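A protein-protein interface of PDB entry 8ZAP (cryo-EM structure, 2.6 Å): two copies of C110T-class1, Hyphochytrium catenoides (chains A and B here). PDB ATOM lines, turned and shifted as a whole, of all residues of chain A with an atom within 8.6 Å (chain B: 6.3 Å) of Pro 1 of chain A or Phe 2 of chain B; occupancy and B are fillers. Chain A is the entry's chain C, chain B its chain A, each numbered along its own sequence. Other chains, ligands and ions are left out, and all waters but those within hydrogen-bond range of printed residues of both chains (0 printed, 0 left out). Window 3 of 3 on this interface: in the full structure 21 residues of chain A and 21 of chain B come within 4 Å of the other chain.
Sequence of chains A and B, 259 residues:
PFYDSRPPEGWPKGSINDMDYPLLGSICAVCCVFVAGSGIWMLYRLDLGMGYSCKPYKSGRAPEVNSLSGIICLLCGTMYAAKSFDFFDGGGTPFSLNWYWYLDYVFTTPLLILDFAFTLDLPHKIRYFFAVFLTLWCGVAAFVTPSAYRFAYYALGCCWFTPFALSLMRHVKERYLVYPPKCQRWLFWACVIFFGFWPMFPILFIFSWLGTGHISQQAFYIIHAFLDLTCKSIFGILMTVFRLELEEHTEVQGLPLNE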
ATOM      1  N   PRO A   1      -3.328 -33.846  32.928  1.00  0.00           N
ATOM      2  CA  PRO A   1      -3.732 -32.957  31.839  1.00  0.00           C
ATOM      3  C   PRO A   1      -2.562 -32.202  31.226  1.00  0.00           C
ATOM      4  O   PRO A   1      -2.718 -31.539  30.202  1.00  0.00           O
ATOM      5  CB  PRO A   1      -4.700 -31.981  32.522  1.00  0.00           C
ATOM      6  CG  PRO A   1      -5.068 -32.615  33.851  1.00  0.00           C
ATOM      7  CD  PRO A   1      -4.364 -33.934  33.966  1.00  0.00           C
ATOM      8  N   PHE A   2      -1.400 -32.313  31.854  1.00  0.00           N
ATOM      9  CA  PHE A   2      -0.261 -31.485  31.495  1.00  0.00           C
ATOM     10  C   PHE A   2       0.373 -31.919  30.182  1.00  0.00           C
ATOM     11  O   PHE A   2       0.581 -33.108  29.929  1.00  0.00           O
ATOM     12  CB  PHE A   2       0.788 -31.516  32.603  1.00  0.00           C
ATOM     13  CG  PHE A   2       1.030 -30.186  33.243  1.00  0.00           C
ATOM     14  CD1 PHE A   2       1.489 -29.119  32.494  1.00  0.00           C
ATOM     15  CD2 PHE A   2       0.820 -30.003  34.593  1.00  0.00           C
ATOM     16  CE1 PHE A   2       1.728 -27.899  33.077  1.00  0.00           C
ATOM     17  CE2 PHE A   2       1.056 -28.784  35.177  1.00  0.00           C
ATOM     18  CZ  PHE A   2       1.516 -27.734  34.420  1.00  0.00           C
ATOM     19  N   TYR A   3       0.678 -30.939  29.359  1.00  0.00           N
ATOM     20  CA  TYR A   3       1.499 -31.050  28.162  1.00  0.00           C
ATOM     21  C   TYR A   3       2.749 -30.192  28.258  1.00  0.00           C
ATOM     22  O   TYR A   3       3.812 -30.607  27.792  1.00  0.00           O
ATOM     23  CB  TYR A   3       0.678 -30.650  26.920  1.00  0.00           C
ATOM     24  CG  TYR A   3       1.461 -30.633  25.624  1.00  0.00           C
ATOM     25  CD1 TYR A   3       1.536 -31.763  24.825  1.00  0.00           C
ATOM     26  CD2 TYR A   3       2.110 -29.483  25.192  1.00  0.00           C
ATOM     27  CE1 TYR A   3       2.244 -31.755  23.643  1.00  0.00           C
ATOM     28  CE2 TYR A   3       2.821 -29.467  24.011  1.00  0.00           C
ATOM     29  CZ  TYR A   3       2.884 -30.606  23.240  1.00  0.00           C
ATOM     30  OH  TYR A   3       3.589 -30.596  22.060  1.00  0.00           O
ATOM     31  N   ASP A   4       2.648 -29.012  28.861  1.00  0.00           N
ATOM     32  CA  ASP A   4       3.765 -28.092  28.956  1.00  0.00           C
ATOM     33  C   ASP A   4       4.623 -28.401  30.177  1.00  0.00           C
ATOM     34  O   ASP A   4       4.221 -29.123  31.092  1.00  0.00           O
ATOM     35  CB  ASP A   4       3.272 -26.646  29.028  1.00  0.00           C
ATOM     36  CG  ASP A   4       2.077 -26.394  28.137  1.00  0.00           C
ATOM     37  OD1 ASP A   4       2.279 -26.134  26.932  1.00  0.00           O
ATOM     38  OD2 ASP A   4       0.936 -26.456  28.639  1.00  0.00           O
ATOM     39  N   PRO A  94       4.671 -31.303  36.979  1.00  0.00           N
ATOM     40  CA  PRO A  94       3.604 -32.165  36.448  1.00  0.00           C
ATOM     41  C   PRO A  94       2.339 -32.156  37.292  1.00  0.00           C
ATOM     42  O   PRO A  94       1.232 -32.143  36.749  1.00  0.00           O
ATOM     43  CB  PRO A  94       4.255 -33.552  36.437  1.00  0.00           C
ATOM     44  CG  PRO A  94       5.701 -33.282  36.266  1.00  0.00           C
ATOM     45  CD  PRO A  94       5.998 -31.934  36.864  1.00  0.00           C
ATOM     46  N   PHE A  95       2.480 -32.161  38.616  1.00  0.00           N
ATOM     47  CA  PHE A  95       1.338 -31.994  39.510  1.00  0.00           C
ATOM     48  C   PHE A  95       1.328 -30.548  39.996  1.00  0.00           C
ATOM     49  O   PHE A  95       1.685 -30.236  41.130  1.00  0.00           O
ATOM     50  CB  PHE A  95       1.393 -32.981  40.669  1.00  0.00           C
ATOM     51  CG  PHE A  95       0.059 -33.235  41.305  1.00  0.00           C
ATOM     52  CD1 PHE A  95      -0.738 -34.284  40.877  1.00  0.00           C
ATOM     53  CD2 PHE A  95      -0.408 -32.417  42.319  1.00  0.00           C
ATOM     54  CE1 PHE A  95      -1.968 -34.516  41.456  1.00  0.00           C
ATOM     55  CE2 PHE A  95      -1.637 -32.646  42.903  1.00  0.00           C
ATOM     56  CZ  PHE A  95      -2.418 -33.697  42.470  1.00  0.00           C
ATOM     57  N   SER A  96       0.907 -29.654  39.111  1.00  0.00           N
ATOM     58  CA  SER A  96       0.814 -28.237  39.421  1.00  0.00           C
ATOM     59  C   SER A  96      -0.644 -27.884  39.673  1.00  0.00           C
ATOM     60  O   SER A  96      -1.477 -27.979  38.765  1.00  0.00           O
ATOM     61  CB  SER A  96       1.385 -27.386  38.290  1.00  0.00           C
ATOM     62  OG  SER A  96       1.356 -26.010  38.617  1.00  0.00           O
ATOM     63  N   TRP A  99      -1.205 -24.251  37.763  1.00  0.00           N
ATOM     64  CA  TRP A  99      -1.235 -24.069  36.317  1.00  0.00           C
ATOM     65  C   TRP A  99      -2.639 -23.754  35.819  1.00  0.00           C
ATOM     66  O   TRP A  99      -2.897 -22.673  35.280  1.00  0.00           O
ATOM     67  CB  TRP A  99      -0.693 -25.317  35.623  1.00  0.00           C
ATOM     68  CG  TRP A  99      -0.343 -25.073  34.197  1.00  0.00           C
ATOM     69  CD1 TRP A  99      -1.087 -25.402  33.105  1.00  0.00           C
ATOM     70  CD2 TRP A  99       0.840 -24.443  33.701  1.00  0.00           C
ATOM     71  NE1 TRP A  99      -0.441 -25.015  31.958  1.00  0.00           N
ATOM     72  CE2 TRP A  99       0.746 -24.424  32.297  1.00  0.00           C
ATOM     73  CE3 TRP A  99       1.973 -23.894  34.309  1.00  0.00           C
ATOM     74  CZ2 TRP A  99       1.739 -23.879  31.491  1.00  0.00           C
ATOM     75  CZ3 TRP A  99       2.955 -23.352  33.508  1.00  0.00           C
ATOM     76  CH2 TRP A  99       2.832 -23.348  32.115  1.00  0.00           C
ATOM     77  N   TYR A 100      -3.558 -24.699  35.983  1.00  0.00           N
ATOM     78  CA  TYR A 100      -4.923 -24.543  35.502  1.00  0.00           C
ATOM     79  C   TYR A 100      -5.699 -23.720  36.520  1.00  0.00           C
ATOM     80  O   TYR A 100      -6.040 -24.214  37.599  1.00  0.00           O
ATOM     81  CB  TYR A 100      -5.568 -25.903  35.263  1.00  0.00           C
ATOM     82  CG  TYR A 100      -4.809 -26.743  34.268  1.00  0.00           C
ATOM     83  CD1 TYR A 100      -4.822 -26.430  32.916  1.00  0.00           C
ATOM     84  CD2 TYR A 100      -4.067 -27.841  34.677  1.00  0.00           C
ATOM     85  CE1 TYR A 100      -4.127 -27.186  32.002  1.00  0.00           C
ATOM     86  CE2 TYR A 100      -3.366 -28.604  33.769  1.00  0.00           C
ATOM     87  CZ  TYR A 100      -3.401 -28.271  32.432  1.00  0.00           C
ATOM     88  OH  TYR A 100      -2.707 -29.026  31.519  1.00  0.00           O
ATOM     89  N   LEU A 103      -9.072 -24.658  38.565  1.00  0.00           N
ATOM     90  CA  LEU A 103      -9.207 -26.109  38.635  1.00  0.00           C
ATOM     91  C   LEU A 103      -9.280 -26.578  40.080  1.00  0.00           C
ATOM     92  O   LEU A 103     -10.060 -27.478  40.406  1.00  0.00           O
ATOM     93  CB  LEU A 103      -8.046 -26.789  37.910  1.00  0.00           C
ATOM     94  CG  LEU A 103      -8.154 -28.310  37.782  1.00  0.00           C
ATOM     95  CD1 LEU A 103      -9.529 -28.716  37.271  1.00  0.00           C
ATOM     96  CD2 LEU A 103      -7.058 -28.866  36.890  1.00  0.00           C
ATOM     97  N   TRP A 137     -16.002 -24.587  36.064  1.00  0.00           N
ATOM     98  CA  TRP A 137     -15.508 -25.272  34.876  1.00  0.00           C
ATOM     99  C   TRP A 137     -15.484 -24.368  33.651  1.00  0.00           C
ATOM    100  O   TRP A 137     -14.575 -24.494  32.823  1.00  0.00           O
ATOM    101  CB  TRP A 137     -16.340 -26.522  34.603  1.00  0.00           C
ATOM    102  CG  TRP A 137     -15.805 -27.709  35.324  1.00  0.00           C
ATOM    103  CD1 TRP A 137     -16.413 -28.398  36.327  1.00  0.00           C
ATOM    104  CD2 TRP A 137     -14.534 -28.336  35.118  1.00  0.00           C
ATOM    105  NE1 TRP A 137     -15.607 -29.422  36.752  1.00  0.00           N
ATOM    106  CE2 TRP A 137     -14.447 -29.407  36.026  1.00  0.00           C
ATOM    107  CE3 TRP A 137     -13.465 -28.101  34.248  1.00  0.00           C
ATOM    108  CZ2 TRP A 137     -13.334 -30.241  36.092  1.00  0.00           C
ATOM    109  CZ3 TRP A 137     -12.363 -28.928  34.315  1.00  0.00           C
ATOM    110  CH2 TRP A 137     -12.306 -29.985  35.230  1.00  0.00           C
ATOM    111  N   VAL A 140     -12.316 -22.492  34.113  1.00  0.00           N
ATOM    112  CA  VAL A 140     -11.177 -23.319  33.723  1.00  0.00           C
ATOM    113  C   VAL A 140     -11.041 -23.352  32.206  1.00  0.00           C
ATOM    114  O   VAL A 140      -9.939 -23.197  31.659  1.00  0.00           O
ATOM    115  CB  VAL A 140     -11.330 -24.737  34.306  1.00  0.00           C
ATOM    116  CG1 VAL A 140     -10.292 -25.678  33.713  1.00  0.00           C
ATOM    117  CG2 VAL A 140     -11.228 -24.706  35.817  1.00  0.00           C
ATOM    118  N   VAL A 144      -7.902 -21.963  29.906  1.00  0.00           N
ATOM    119  CA  VAL A 144      -7.117 -22.837  29.037  1.00  0.00           C
ATOM    120  C   VAL A 144      -7.343 -22.559  27.555  1.00  0.00           C
ATOM    121  O   VAL A 144      -6.649 -23.153  26.715  1.00  0.00           O
ATOM    122  CB  VAL A 144      -7.384 -24.331  29.325  1.00  0.00           C
ATOM    123  CG1 VAL A 144      -7.065 -24.658  30.772  1.00  0.00           C
ATOM    124  CG2 VAL A 144      -8.812 -24.703  28.972  1.00  0.00           C
ATOM    125  N   PRO B   1      -6.196 -33.389  29.785  1.00  0.00           N
ATOM    126  CA  PRO B   1      -5.788 -34.663  29.193  1.00  0.00           C
ATOM    127  C   PRO B   1      -5.214 -34.507  27.793  1.00  0.00           C
ATOM    128  O   PRO B   1      -4.688 -35.465  27.228  1.00  0.00           O
ATOM    129  CB  PRO B   1      -7.095 -35.465  29.150  1.00  0.00           C
ATOM    130  CG  PRO B   1      -8.065 -34.739  30.066  1.00  0.00           C
ATOM    131  CD  PRO B   1      -7.370 -33.550  30.656  1.00  0.00           C
ATOM    132  N   PHE B   2      -5.316 -33.303  27.248  1.00  0.00           N
ATOM    133  CA  PHE B   2      -4.998 -33.074  25.848  1.00  0.00           C
ATOM    134  C   PHE B   2      -3.499 -33.098  25.588  1.00  0.00           C
ATOM    135  O   PHE B   2      -2.707 -32.514  26.333  1.00  0.00           O
ATOM    136  CB  PHE B   2      -5.575 -31.740  25.383  1.00  0.00           C
ATOM    137  CG  PHE B   2      -6.608 -31.872  24.308  1.00  0.00           C
ATOM    138  CD1 PHE B   2      -6.285 -32.446  23.092  1.00  0.00           C
ATOM    139  CD2 PHE B   2      -7.890 -31.407  24.499  1.00  0.00           C
ATOM    140  CE1 PHE B   2      -7.222 -32.556  22.095  1.00  0.00           C
ATOM    141  CE2 PHE B   2      -8.829 -31.519  23.505  1.00  0.00           C
ATOM    142  CZ  PHE B   2      -8.493 -32.088  22.301  1.00  0.00           C
ATOM    143  N   TYR B   3      -3.128 -33.774  24.523  1.00  0.00           N
ATOM    144  CA  TYR B   3      -1.805 -33.758  23.915  1.00  0.00           C
ATOM    145  C   TYR B   3      -1.850 -33.231  22.492  1.00  0.00           C
ATOM    146  O   TYR B   3      -0.933 -32.519  22.075  1.00  0.00           O
ATOM    147  CB  TYR B   3      -1.199 -35.176  23.935  1.00  0.00           C
ATOM    148  CG  TYR B   3       0.139 -35.300  23.238  1.00  0.00           C
ATOM    149  CD1 TYR B   3       1.323 -35.121  23.936  1.00  0.00           C
ATOM    150  CD2 TYR B   3       0.218 -35.613  21.886  1.00  0.00           C
ATOM    151  CE1 TYR B   3       2.545 -35.237  23.310  1.00  0.00           C
ATOM    152  CE2 TYR B   3       1.436 -35.728  21.252  1.00  0.00           C
ATOM    153  CZ  TYR B   3       2.597 -35.540  21.969  1.00  0.00           C
ATOM    154  OH  TYR B   3       3.816 -35.656  21.344  1.00  0.00           O
ATOM    155  N   ASP B   4      -2.899 -33.554  21.743  1.00  0.00           N
ATOM    156  CA  ASP B   4      -3.013 -33.151  20.353  1.00  0.00           C
ATOM    157  C   ASP B   4      -3.623 -31.760  20.240  1.00  0.00           C
ATOM    158  O   ASP B   4      -4.213 -31.225  21.182  1.00  0.00           O
ATOM    159  CB  ASP B   4      -3.862 -34.151  19.567  1.00  0.00           C
ATOM    160  CG  ASP B   4      -3.598 -35.582  19.972  1.00  0.00           C
ATOM    161  OD1 ASP B   4      -4.342 -36.104  20.827  1.00  0.00           O
ATOM    162  OD2 ASP B   4      -2.645 -36.186  19.437  1.00  0.00           O
ATOM    163  N   SER B   5      -3.466 -31.174  19.058  1.00  0.00           N
ATOM    164  CA  SER B   5      -4.044 -29.879  18.748  1.00  0.00           C
ATOM    165  C   SER B   5      -4.242 -29.798  17.245  1.00  0.00           C
ATOM    166  O   SER B   5      -3.654 -30.567  16.481  1.00  0.00           O
ATOM    167  CB  SER B   5      -3.160 -28.731  19.247  1.00  0.00           C
ATOM    168  OG  SER B   5      -1.813 -28.920  18.857  1.00  0.00           O
ATOM    169  N   ASP B  86     -15.962 -25.112  20.869  1.00  0.00           N
ATOM    170  CA  ASP B  86     -14.855 -25.898  20.333  1.00  0.00           C
ATOM    171  C   ASP B  86     -14.966 -26.064  18.822  1.00  0.00           C
ATOM    172  O   ASP B  86     -13.975 -25.913  18.100  1.00  0.00           O
ATOM    173  CB  ASP B  86     -14.808 -27.263  21.020  1.00  0.00           C
ATOM    174  CG  ASP B  86     -14.023 -28.291  20.229  1.00  0.00           C
ATOM    175  OD1 ASP B  86     -12.779 -28.280  20.308  1.00  0.00           O
ATOM    176  OD2 ASP B  86     -14.647 -29.115  19.531  1.00  0.00           O
ATOM    177  N   GLY B  92     -10.249 -29.440  18.154  1.00  0.00           N
ATOM    178  CA  GLY B  92      -8.939 -29.648  18.739  1.00  0.00           C
ATOM    179  C   GLY B  92      -8.524 -28.597  19.740  1.00  0.00           C
ATOM    180  O   GLY B  92      -7.329 -28.441  20.005  1.00  0.00           O
ATOM    181  N   THR B  93      -9.480 -27.869  20.300  1.00  0.00           N
ATOM    182  CA  THR B  93      -9.392 -26.840  21.326  1.00  0.00           C
ATOM    183  C   THR B  93      -8.964 -27.473  22.648  1.00  0.00           C
ATOM    184  O   THR B  93      -9.389 -28.587  22.959  1.00  0.00           O
ATOM    185  CB  THR B  93     -10.741 -26.137  21.481  1.00  0.00           C
ATOM    186  OG1 THR B  93     -10.952 -25.264  20.364  1.00  0.00           O
ATOM    187  CG2 THR B  93     -10.822 -25.329  22.771  1.00  0.00           C
ATOM    188  N   PRO B  94      -8.099 -26.814  23.437  1.00  0.00           N
ATOM    189  CA  PRO B  94      -7.622 -27.430  24.684  1.00  0.00           C
ATOM    190  C   PRO B  94      -8.744 -27.897  25.600  1.00  0.00           C
ATOM    191  O   PRO B  94      -8.645 -28.968  26.203  1.00  0.00           O
ATOM    192  CB  PRO B  94      -6.807 -26.307  25.334  1.00  0.00           C
ATOM    193  CG  PRO B  94      -6.322 -25.492  24.197  1.00  0.00           C
ATOM    194  CD  PRO B  94      -7.320 -25.616  23.077  1.00  0.00           C
ATOM    195  N   PHE B  95      -9.813 -27.111  25.718  1.00  0.00           N
ATOM    196  CA  PHE B  95     -11.007 -27.542  26.438  1.00  0.00           C
ATOM    197  C   PHE B  95     -12.042 -27.992  25.412  1.00  0.00           C
ATOM    198  O   PHE B  95     -13.014 -27.300  25.117  1.00  0.00           O
ATOM    199  CB  PHE B  95     -11.542 -26.431  27.334  1.00  0.00           C
ATOM    200  CG  PHE B  95     -12.405 -26.930  28.456  1.00  0.00           C
ATOM    201  CD1 PHE B  95     -11.855 -27.218  29.693  1.00  0.00           C
ATOM    202  CD2 PHE B  95     -13.763 -27.124  28.270  1.00  0.00           C
ATOM    203  CE1 PHE B  95     -12.646 -27.680  30.726  1.00  0.00           C
ATOM    204  CE2 PHE B  95     -14.557 -27.587  29.299  1.00  0.00           C
ATOM    205  CZ  PHE B  95     -13.998 -27.865  30.528  1.00  0.00           C
ATOM    206  N   SER B  96     -11.819 -29.177  24.861  1.00  0.00           N
ATOM    207  CA  SER B  96     -12.718 -29.760  23.879  1.00  0.00           C
ATOM    208  C   SER B  96     -13.559 -30.831  24.558  1.00  0.00           C
ATOM    209  O   SER B  96     -13.026 -31.847  25.016  1.00  0.00           O
ATOM    210  CB  SER B  96     -11.945 -30.350  22.702  1.00  0.00           C
ATOM    211  OG  SER B  96     -12.820 -30.853  21.712  1.00  0.00           O
ATOM    212  N   LEU B  97     -14.866 -30.597  24.627  1.00  0.00           N
ATOM    213  CA  LEU B  97     -15.812 -31.592  25.102  1.00  0.00           C
ATOM    214  C   LEU B  97     -16.288 -32.499  23.978  1.00  0.00           C
ATOM    215  O   LEU B  97     -17.157 -33.349  24.197  1.00  0.00           O
ATOM    216  CB  LEU B  97     -16.996 -30.908  25.785  1.00  0.00           C
ATOM    217  CG  LEU B  97     -16.648 -30.260  27.125  1.00  0.00           C
ATOM    218  CD1 LEU B  97     -17.893 -29.780  27.830  1.00  0.00           C
ATOM    219  CD2 LEU B  97     -15.876 -31.226  28.007  1.00  0.00           C
ATOM    220  N   TRP B  99     -13.698 -33.945  21.832  1.00  0.00           N
ATOM    221  CA  TRP B  99     -12.567 -34.804  21.493  1.00  0.00           C
ATOM    222  C   TRP B  99     -12.739 -36.209  22.050  1.00  0.00           C
ATOM    223  O   TRP B  99     -12.837 -37.185  21.299  1.00  0.00           O
ATOM    224  CB  TRP B  99     -11.269 -34.183  22.008  1.00  0.00           C
ATOM    225  CG  TRP B  99     -10.060 -34.789  21.389  1.00  0.00           C
ATOM    226  CD1 TRP B  99      -9.242 -35.728  21.941  1.00  0.00           C
ATOM    227  CD2 TRP B  99      -9.528 -34.506  20.092  1.00  0.00           C
ATOM    228  NE1 TRP B  99      -8.233 -36.048  21.070  1.00  0.00           N
ATOM    229  CE2 TRP B  99      -8.385 -35.309  19.926  1.00  0.00           C
ATOM    230  CE3 TRP B  99      -9.906 -33.648  19.057  1.00  0.00           C
ATOM    231  CZ2 TRP B  99      -7.618 -35.281  18.767  1.00  0.00           C
ATOM    232  CZ3 TRP B  99      -9.144 -33.623  17.908  1.00  0.00           C
ATOM    233  CH2 TRP B  99      -8.013 -34.433  17.772  1.00  0.00           C
ATOM    234  N   TYR B 100     -12.769 -36.330  23.372  1.00  0.00           N
ATOM    235  CA  TYR B 100     -12.877 -37.626  24.028  1.00  0.00           C
ATOM    236  C   TYR B 100     -14.341 -38.041  24.032  1.00  0.00           C
ATOM    237  O   TYR B 100     -15.147 -37.498  24.793  1.00  0.00           O
ATOM    238  CB  TYR B 100     -12.302 -37.563  25.440  1.00  0.00           C
ATOM    239  CG  TYR B 100     -10.855 -37.137  25.462  1.00  0.00           C
ATOM    240  CD1 TYR B 100      -9.857 -37.997  25.029  1.00  0.00           C
ATOM    241  CD2 TYR B 100     -10.488 -35.876  25.903  1.00  0.00           C
ATOM    242  CE1 TYR B 100      -8.536 -37.617  25.038  1.00  0.00           C
ATOM    243  CE2 TYR B 100      -9.167 -35.485  25.914  1.00  0.00           C
ATOM    244  CZ  TYR B 100      -8.194 -36.360  25.482  1.00  0.00           C
ATOM    245  OH  TYR B 100      -6.874 -35.981  25.491  1.00  0.00           O
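Among the printed residues, pairs that only touch across the chains: Pro 1 of chain A with Pro 1 of chain B, Val 144 of chain A with Pro 94 of chain B, Tyr 3 of chain A with Tyr 3 of chain B, Val 144 of chain A with Phe 95 of chain B, Trp 137 of chain A with Phe 95 of chain B, Tyr 3 of chain A with Phe 2 of chain B and Pro 1 of chain A with Phe 2 of chain B.
The backbone carbonyl oxygen of Pro 1 of chain A is in hydrogen-bond range of the side-chain hydroxyl of Tyr 100 of chain A, 2.8 Å away. The backbone carbonyl oxygen of Pro 1 of chain B sits at hydrogen-bond distance from the side-chain hydroxyl of Tyr 100 of chain B, 2.8 Å away.
Of the printed residues of chain B, Pro 1 of chain A touches Pro 1 (3.2 Å) and Phe 2 (3.99 Å). Printed residues of chain A within 4 Å of Phe 2 of chain B: Pro 1 and Tyr 3. Of chain A, only Pro 1 comes within 4 Å of Pro 1 of chain B. Printed residues of chain A within 4 Å of Phe 95 of chain B: Trp 137 and Val 144. Printed residues of chain A within 4 Å of Pro 94 of chain B: Val 144. Asp 4 of chain B touches none of the printed residues of chain A. The nearest printed residue of chain B that does not touch Pro 1 of chain A is Tyr 3 of chain B (6.1 Å). The nearest printed residue of chain B that does not touch Val 144 of chain A is Thr 93 of chain B (6.1 Å).
Of the 13 printed residues of chain A, 4 touch a printed residue of chain B. Hydrophobic or aromatic side chains of chain A within 4 Å of the printed part of chain B: Pro 1, Tyr 3, Trp 137 and Val 144. Hydrophobic or aromatic side chains of chain B that line the printed part of chain A: Pro 1, Tyr 3, Pro 94 and Phe 95. Along chain B the printed residues that touch a printed residue of chain A span positions 1 to 95. Among the printed residues, no Asp or Glu carboxylate lies within 4 Å of a Lys or Arg side-chain nitrogen of the other chain.
Pro 1 of chain A touches its own counterpart, Pro 1 of chain B. Pro 1 of chain A touches Phe 2 of chain B, but with the chains exchanged Phe 2 of chain A does not touch Pro 1 of chain B (5.3 Å). Tyr 3 of chain A touches Phe 2 of chain B, but with the chains exchanged Phe 2 of chain A does not touch Tyr 3 of chain B (6.4 Å). Tyr 3 of chain B touches its own counterpart, Tyr 3 of chain A. 9 positions are printed for both chains. Of the 7 pairs that touch across the chains among the printed residues, 2 have their exchanged pair printed and touching as well.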
